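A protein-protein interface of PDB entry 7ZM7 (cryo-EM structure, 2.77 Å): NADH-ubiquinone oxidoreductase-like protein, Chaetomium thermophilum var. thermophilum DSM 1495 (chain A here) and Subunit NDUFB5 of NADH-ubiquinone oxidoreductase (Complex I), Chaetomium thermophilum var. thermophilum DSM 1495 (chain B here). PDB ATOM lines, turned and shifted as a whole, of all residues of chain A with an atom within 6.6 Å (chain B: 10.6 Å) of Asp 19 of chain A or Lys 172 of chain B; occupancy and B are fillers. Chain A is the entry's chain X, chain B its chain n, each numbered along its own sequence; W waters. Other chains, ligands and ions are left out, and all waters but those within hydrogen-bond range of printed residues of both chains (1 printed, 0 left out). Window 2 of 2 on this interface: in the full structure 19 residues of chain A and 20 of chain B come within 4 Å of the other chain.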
ATOM      1  N   VAL A  16      16.161 -24.858   1.189  1.00  0.00           N
ATOM      2  CA  VAL A  16      17.001 -23.729   0.716  1.00  0.00           C
ATOM      3  C   VAL A  16      17.584 -23.048   1.947  1.00  0.00           C
ATOM      4  O   VAL A  16      16.829 -22.809   2.891  1.00  0.00           O
ATOM      5  CB  VAL A  16      16.246 -22.770  -0.208  1.00  0.00           C
ATOM      6  CG1 VAL A  16      17.182 -21.722  -0.783  1.00  0.00           C
ATOM      7  CG2 VAL A  16      15.559 -23.523  -1.332  1.00  0.00           C
ATOM      8  N   LYS A  17      18.878 -22.710   1.902  1.00  0.00           N
ATOM      9  CA  LYS A  17      19.555 -21.929   2.964  1.00  0.00           C
ATOM     10  C   LYS A  17      19.089 -20.472   2.919  1.00  0.00           C
ATOM     11  O   LYS A  17      19.481 -19.762   1.986  1.00  0.00           O
ATOM     12  CB  LYS A  17      21.077 -22.005   2.808  1.00  0.00           C
ATOM     13  CG  LYS A  17      21.872 -21.411   3.963  1.00  0.00           C
ATOM     14  CD  LYS A  17      23.366 -21.494   3.769  1.00  0.00           C
ATOM     15  CE  LYS A  17      24.143 -20.805   4.871  1.00  0.00           C
ATOM     16  NZ  LYS A  17      25.605 -20.873   4.638  1.00  0.00           N
ATOM     17  N   THR A  18      18.278 -20.057   3.880  1.00  0.00           N
ATOM     18  CA  THR A  18      17.739 -18.682   3.958  1.00  0.00           C
ATOM     19  C   THR A  18      17.917 -18.240   5.408  1.00  0.00           C
ATOM     20  O   THR A  18      18.334 -19.078   6.214  1.00  0.00           O
ATOM     21  CB  THR A  18      16.259 -18.628   3.553  1.00  0.00           C
ATOM     22  OG1 THR A  18      15.463 -19.119   4.633  1.00  0.00           O
ATOM     23  CG2 THR A  18      15.936 -19.375   2.277  1.00  0.00           C
ATOM     24  N   ASP A  19      17.709 -16.962   5.710  1.00  0.00           N
ATOM     25  CA  ASP A  19      17.942 -16.436   7.078  1.00  0.00           C
ATOM     26  C   ASP A  19      16.707 -16.487   7.970  1.00  0.00           C
ATOM     27  O   ASP A  19      16.859 -16.188   9.151  1.00  0.00           O
ATOM     28  CB  ASP A  19      18.332 -14.964   7.000  1.00  0.00           C
ATOM     29  CG  ASP A  19      19.748 -14.748   6.494  1.00  0.00           C
ATOM     30  OD1 ASP A  19      20.395 -15.743   6.112  1.00  0.00           O
ATOM     31  OD2 ASP A  19      20.195 -13.585   6.495  1.00  0.00           O
ATOM     32  N   TYR A  20      15.542 -16.830   7.444  1.00  0.00           N
ATOM     33  CA  TYR A  20      14.289 -16.734   8.239  1.00  0.00           C
ATOM     34  C   TYR A  20      13.446 -17.999   8.067  1.00  0.00           C
ATOM     35  O   TYR A  20      13.621 -18.695   7.069  1.00  0.00           O
ATOM     36  CB  TYR A  20      13.514 -15.484   7.824  1.00  0.00           C
ATOM     37  CG  TYR A  20      14.243 -14.168   7.914  1.00  0.00           C
ATOM     38  CD1 TYR A  20      14.345 -13.489   9.115  1.00  0.00           C
ATOM     39  CD2 TYR A  20      14.793 -13.581   6.788  1.00  0.00           C
ATOM     40  CE1 TYR A  20      15.002 -12.274   9.201  1.00  0.00           C
ATOM     41  CE2 TYR A  20      15.446 -12.363   6.853  1.00  0.00           C
ATOM     42  CZ  TYR A  20      15.549 -11.708   8.064  1.00  0.00           C
ATOM     43  OH  TYR A  20      16.196 -10.509   8.135  1.00  0.00           O
ATOM     44  N   PRO A  21      12.477 -18.273   8.962  1.00  0.00           N
ATOM     45  CA  PRO A  21      11.685 -19.502   8.908  1.00  0.00           C
ATOM     46  C   PRO A  21      10.820 -19.643   7.644  1.00  0.00           C
ATOM     47  O   PRO A  21      10.188 -18.674   7.317  1.00  0.00           O
ATOM     48  CB  PRO A  21      10.867 -19.465  10.205  1.00  0.00           C
ATOM     49  CG  PRO A  21      10.870 -18.023  10.644  1.00  0.00           C
ATOM     50  CD  PRO A  21      12.190 -17.479  10.156  1.00  0.00           C
ATOM     51  N   GLY A 100      10.798 -17.390   3.399  1.00  0.00           N
ATOM     52  CA  GLY A 100      11.823 -17.228   4.447  1.00  0.00           C
ATOM     53  C   GLY A 100      12.974 -16.360   3.994  1.00  0.00           C
ATOM     54  O   GLY A 100      14.023 -16.385   4.647  1.00  0.00           O
ATOM     55  N   MET A 101      12.802 -15.643   2.891  1.00  0.00           N
ATOM     56  CA  MET A 101      13.875 -14.830   2.284  1.00  0.00           C
ATOM     57  C   MET A 101      13.702 -13.373   2.698  1.00  0.00           C
ATOM     58  O   MET A 101      14.453 -12.527   2.199  1.00  0.00           O
ATOM     59  CB  MET A 101      13.795 -15.006   0.770  1.00  0.00           C
ATOM     60  CG  MET A 101      13.554 -16.458   0.411  1.00  0.00           C
ATOM     61  SD  MET A 101      14.069 -16.944  -1.239  1.00  0.00           S
ATOM     62  CE  MET A 101      13.935 -18.725  -1.105  1.00  0.00           C
ATOM     63  N   GLU B 164      16.611 -30.080  10.541  1.00  0.00           N
ATOM     64  CA  GLU B 164      17.912 -29.490  10.932  1.00  0.00           C
ATOM     65  C   GLU B 164      17.986 -28.015  10.520  1.00  0.00           C
ATOM     66  O   GLU B 164      18.462 -27.201  11.329  1.00  0.00           O
ATOM     67  CB  GLU B 164      19.062 -30.259  10.290  1.00  0.00           C
ATOM     68  CG  GLU B 164      20.310 -30.297  11.151  1.00  0.00           C
ATOM     69  CD  GLU B 164      20.167 -31.073  12.450  1.00  0.00           C
ATOM     70  OE1 GLU B 164      19.435 -32.085  12.459  1.00  0.00           O
ATOM     71  OE2 GLU B 164      20.783 -30.661  13.451  1.00  0.00           O
ATOM     72  N   GLU B 165      17.564 -27.677   9.302  1.00  0.00           N
ATOM     73  CA  GLU B 165      17.664 -26.276   8.831  1.00  0.00           C
ATOM     74  C   GLU B 165      16.710 -25.390   9.626  1.00  0.00           C
ATOM     75  O   GLU B 165      17.088 -24.245   9.919  1.00  0.00           O
ATOM     76  CB  GLU B 165      17.449 -26.174   7.326  1.00  0.00           C
ATOM     77  CG  GLU B 165      18.105 -24.962   6.694  1.00  0.00           C
ATOM     78  CD  GLU B 165      19.521 -25.214   6.204  1.00  0.00           C
ATOM     79  OE1 GLU B 165      19.942 -26.385   6.198  1.00  0.00           O
ATOM     80  OE2 GLU B 165      20.196 -24.239   5.827  1.00  0.00           O
ATOM     81  N   GLU B 166      15.524 -25.887   9.943  1.00  0.00           N
ATOM     82  CA  GLU B 166      14.561 -25.124  10.769  1.00  0.00           C
ATOM     83  C   GLU B 166      15.223 -24.846  12.112  1.00  0.00           C
ATOM     84  O   GLU B 166      15.154 -23.705  12.566  1.00  0.00           O
ATOM     85  CB  GLU B 166      13.331 -25.991  11.024  1.00  0.00           C
ATOM     86  CG  GLU B 166      12.186 -25.283  11.719  1.00  0.00           C
ATOM     87  CD  GLU B 166      11.132 -26.257  12.217  1.00  0.00           C
ATOM     88  OE1 GLU B 166       9.995 -25.822  12.485  1.00  0.00           O
ATOM     89  OE2 GLU B 166      11.460 -27.452  12.334  1.00  0.00           O
ATOM     90  N   GLU B 167      15.898 -25.839  12.684  1.00  0.00           N
ATOM     91  CA  GLU B 167      16.609 -25.677  13.976  1.00  0.00           C
ATOM     92  C   GLU B 167      17.733 -24.653  13.870  1.00  0.00           C
ATOM     93  O   GLU B 167      17.857 -23.839  14.775  1.00  0.00           O
ATOM     94  CB  GLU B 167      17.263 -27.000  14.350  1.00  0.00           C
ATOM     95  CG  GLU B 167      16.277 -28.088  14.728  1.00  0.00           C
ATOM     96  CD  GLU B 167      16.871 -29.486  14.703  1.00  0.00           C
ATOM     97  OE1 GLU B 167      18.100 -29.605  14.872  1.00  0.00           O
ATOM     98  OE2 GLU B 167      16.107 -30.451  14.497  1.00  0.00           O
ATOM     99  N   ARG B 168      18.514 -24.688  12.806  1.00  0.00           N
ATOM    100  CA  ARG B 168      19.680 -23.775  12.762  1.00  0.00           C
ATOM    101  C   ARG B 168      19.169 -22.343  12.814  1.00  0.00           C
ATOM    102  O   ARG B 168      19.687 -21.590  13.638  1.00  0.00           O
ATOM    103  CB  ARG B 168      20.565 -24.070  11.542  1.00  0.00           C
ATOM    104  CG  ARG B 168      21.753 -23.138  11.348  1.00  0.00           C
ATOM    105  CD  ARG B 168      21.455 -21.922  10.490  1.00  0.00           C
ATOM    106  NE  ARG B 168      20.834 -22.276   9.222  1.00  0.00           N
ATOM    107  CZ  ARG B 168      20.267 -21.407   8.394  1.00  0.00           C
ATOM    108  NH1 ARG B 168      19.729 -21.824   7.262  1.00  0.00           N
ATOM    109  NH2 ARG B 168      20.223 -20.124   8.707  1.00  0.00           N
ATOM    110  N   LYS B 169      18.179 -22.004  11.994  1.00  0.00           N
ATOM    111  CA  LYS B 169      17.677 -20.611  11.954  1.00  0.00           C
ATOM    112  C   LYS B 169      17.024 -20.324  13.290  1.00  0.00           C
ATOM    113  O   LYS B 169      17.220 -19.237  13.822  1.00  0.00           O
ATOM    114  CB  LYS B 169      16.591 -20.428  10.894  1.00  0.00           C
ATOM    115  CG  LYS B 169      16.944 -20.813   9.466  1.00  0.00           C
ATOM    116  CD  LYS B 169      15.735 -20.789   8.565  1.00  0.00           C
ATOM    117  CE  LYS B 169      16.014 -21.240   7.150  1.00  0.00           C
ATOM    118  NZ  LYS B 169      14.756 -21.378   6.382  1.00  0.00           N
ATOM    119  N   ALA B 170      16.251 -21.282  13.784  1.00  0.00           N
ATOM    120  CA  ALA B 170      15.601 -21.116  15.094  1.00  0.00           C
ATOM    121  C   ALA B 170      16.687 -20.797  16.114  1.00  0.00           C
ATOM    122  O   ALA B 170      16.539 -19.816  16.843  1.00  0.00           O
ATOM    123  CB  ALA B 170      14.850 -22.368  15.458  1.00  0.00           C
ATOM    124  N   LYS B 171      17.738 -21.599  16.143  1.00  0.00           N
ATOM    125  CA  LYS B 171      18.785 -21.361  17.120  1.00  0.00           C
ATOM    126  C   LYS B 171      19.576 -20.097  16.829  1.00  0.00           C
ATOM    127  O   LYS B 171      20.325 -19.644  17.699  1.00  0.00           O
ATOM    128  CB  LYS B 171      19.728 -22.564  17.171  1.00  0.00           C
ATOM    129  CG  LYS B 171      20.431 -22.771  18.502  1.00  0.00           C
ATOM    130  CD  LYS B 171      21.184 -24.094  18.508  1.00  0.00           C
ATOM    131  CE  LYS B 171      22.352 -24.067  17.531  1.00  0.00           C
ATOM    132  NZ  LYS B 171      23.072 -25.369  17.475  1.00  0.00           N
ATOM    133  N   LYS B 172      19.419 -19.511  15.647  1.00  0.00           N
ATOM    134  CA  LYS B 172      20.225 -18.370  15.237  1.00  0.00           C
ATOM    135  C   LYS B 172      19.515 -17.039  15.440  1.00  0.00           C
ATOM    136  O   LYS B 172      20.118 -16.096  15.960  1.00  0.00           O
ATOM    137  CB  LYS B 172      20.652 -18.541  13.774  1.00  0.00           C
ATOM    138  CG  LYS B 172      21.534 -17.440  13.225  1.00  0.00           C
ATOM    139  CD  LYS B 172      20.725 -16.419  12.440  1.00  0.00           C
ATOM    140  CE  LYS B 172      20.226 -17.024  11.129  1.00  0.00           C
ATOM    141  NZ  LYS B 172      19.439 -16.067  10.308  1.00  0.00           N
ATOM    142  N   LEU B 173      18.254 -16.924  15.041  1.00  0.00           N
ATOM    143  CA  LEU B 173      17.544 -15.671  15.245  1.00  0.00           C
ATOM    144  C   LEU B 173      16.747 -15.646  16.540  1.00  0.00           C
ATOM    145  O   LEU B 173      15.987 -14.700  16.763  1.00  0.00           O
ATOM    146  CB  LEU B 173      16.626 -15.356  14.058  1.00  0.00           C
ATOM    147  CG  LEU B 173      15.536 -16.317  13.601  1.00  0.00           C
ATOM    148  CD1 LEU B 173      14.237 -16.044  14.332  1.00  0.00           C
ATOM    149  CD2 LEU B 173      15.346 -16.156  12.097  1.00  0.00           C
ATOM    150  N   ALA B 174      16.887 -16.662  17.388  1.00  0.00           N
ATOM    151  CA  ALA B 174      16.354 -16.603  18.741  1.00  0.00           C
ATOM    152  C   ALA B 174      17.430 -16.430  19.797  1.00  0.00           C
ATOM    153  O   ALA B 174      17.154 -15.855  20.850  1.00  0.00           O
ATOM    154  CB  ALA B 174      15.541 -17.862  19.061  1.00  0.00           C
ATOM    155  N   ALA B 175      18.643 -16.915  19.544  1.00  0.00           N
ATOM    156  CA  ALA B 175      19.762 -16.674  20.442  1.00  0.00           C
ATOM    157  C   ALA B 175      20.490 -15.372  20.142  1.00  0.00           C
ATOM    158  O   ALA B 175      21.312 -14.939  20.956  1.00  0.00           O
ATOM    159  CB  ALA B 175      20.755 -17.839  20.382  1.00  0.00           C
ATOM    160  N   ALA B 176      20.211 -14.741  19.002  1.00  0.00           N
ATOM    161  CA  ALA B 176      20.775 -13.439  18.675  1.00  0.00           C
ATOM    162  C   ALA B 176      19.731 -12.332  18.730  1.00  0.00           C
ATOM    163  O   ALA B 176      20.036 -11.187  18.377  1.00  0.00           O
ATOM    164  CB  ALA B 176      21.437 -13.469  17.295  1.00  0.00           C
ATOM    165  N   ALA B 177      18.511 -12.644  19.162  1.00  0.00           N
ATOM    166  CA  ALA B 177      17.462 -11.652  19.352  1.00  0.00           C
ATOM    167  C   ALA B 177      17.324 -11.245  20.812  1.00  0.00           C
ATOM    168  O   ALA B 177      16.339 -10.601  21.186  1.00  0.00           O
ATOM    169  CB  ALA B 177      16.128 -12.179  18.821  1.00  0.00           C
ATOM    170  N   ALA B 178      18.290 -11.616  21.644  1.00  0.00           N
ATOM    171  CA  ALA B 178      18.265 -11.279  23.059  1.00  0.00           C
ATOM    172  C   ALA B 178      19.623 -10.747  23.502  1.00  0.00           C
ATOM    173  O   ALA B 178      20.656 -11.126  22.953  1.00  0.00           O
ATOM    174  CB  ALA B 178      17.871 -12.492  23.886  1.00  0.00           C
HETATM  175  O   HOH W   1      13.830 -22.152   3.342  1.00  0.00           O
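Water W1 bridges the backbone carbonyl oxygen (O) of Val 16 of chain A (3.1 Å) and the side-chain amino group (NZ) of Lys 169 of chain B (3.3 Å).
Of the 8 printed residues of chain A, 5 touch a printed residue of chain B. Hydrophobic or aromatic side chains of chain A that line the printed part of chain B: Pro 21. Of the 15 printed residues of chain B, 5 touch a printed residue of chain A. Hydrophobic or aromatic side chains of chain B within 4 Å of the printed part of chain A: Leu 173. Among the printed residues, 8 pairs touch across the chains. Among the printed residues, no Asp or Glu carboxylate lies within 4 Å of a Lys or Arg side-chain nitrogen of the other chain.
Among the printed residues, merely in contact across the chains: Asp 19 of chain A with Leu 173 of chain B (3.3 Å), Lys 17 of chain A with Glu 165 of chain B (3.7 Å), Pro 21 of chain A with Leu 173 of chain B (3.9 Å) and Lys 17 of chain A with Arg 168 of chain B (3.96 Å).
Tyr 20 of chain A touches just one residue of chain B: Lys 169. Printed residues of chain A within 4 Å of Arg 168 of chain B: Lys 17 and Thr 18. Printed residues of chain B within 4 Å of Pro 21 of chain A: Leu 173. Printed residues of chain A within 4 Å of Leu 173 of chain B: Asp 19 (3.3 Å) and Pro 21 (3.9 Å). Met 101 of chain A touches none of the printed residues of chain B.
OG1 of Thr 18 of chain A lies within hydrogen-bond range of O of Tyr 20 of chain A, 3.1 Å away. O of Gly 100 of chain A lies within hydrogen-bond range of OG1 of Thr 18 of chain A (3.1 Å). The backbone carbonyl oxygen of Gly 100 of chain A is in hydrogen-bond range of the backbone NH of Tyr 20 of chain A, 3.2 Å away. OE2 of Glu 165 of chain B lies within salt-bridge range of NH1 of Arg 168 of chain B (2.8 Å).
NH1 of Arg 168 of chain B lies within hydrogen-bond range of O of Thr 18 of chain A (3.3 Å). The side-chain hydroxyl (OG1) of Thr 18 of chain A sits at hydrogen-bond distance from the side-chain amino group (NZ) of Lys 169 of chain B (2.9 Å). The backbone carbonyl oxygen (O) of Asp 19 of chain A sits at hydrogen-bond distance from the side-chain amino group (NZ) of Lys 172 of chain B (2.8 Å). The backbone carbonyl oxygen of Tyr 20 of chain A sits at hydrogen-bond distance from the side-chain amino group of Lys 169 of chain B, at 3.0 Å.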
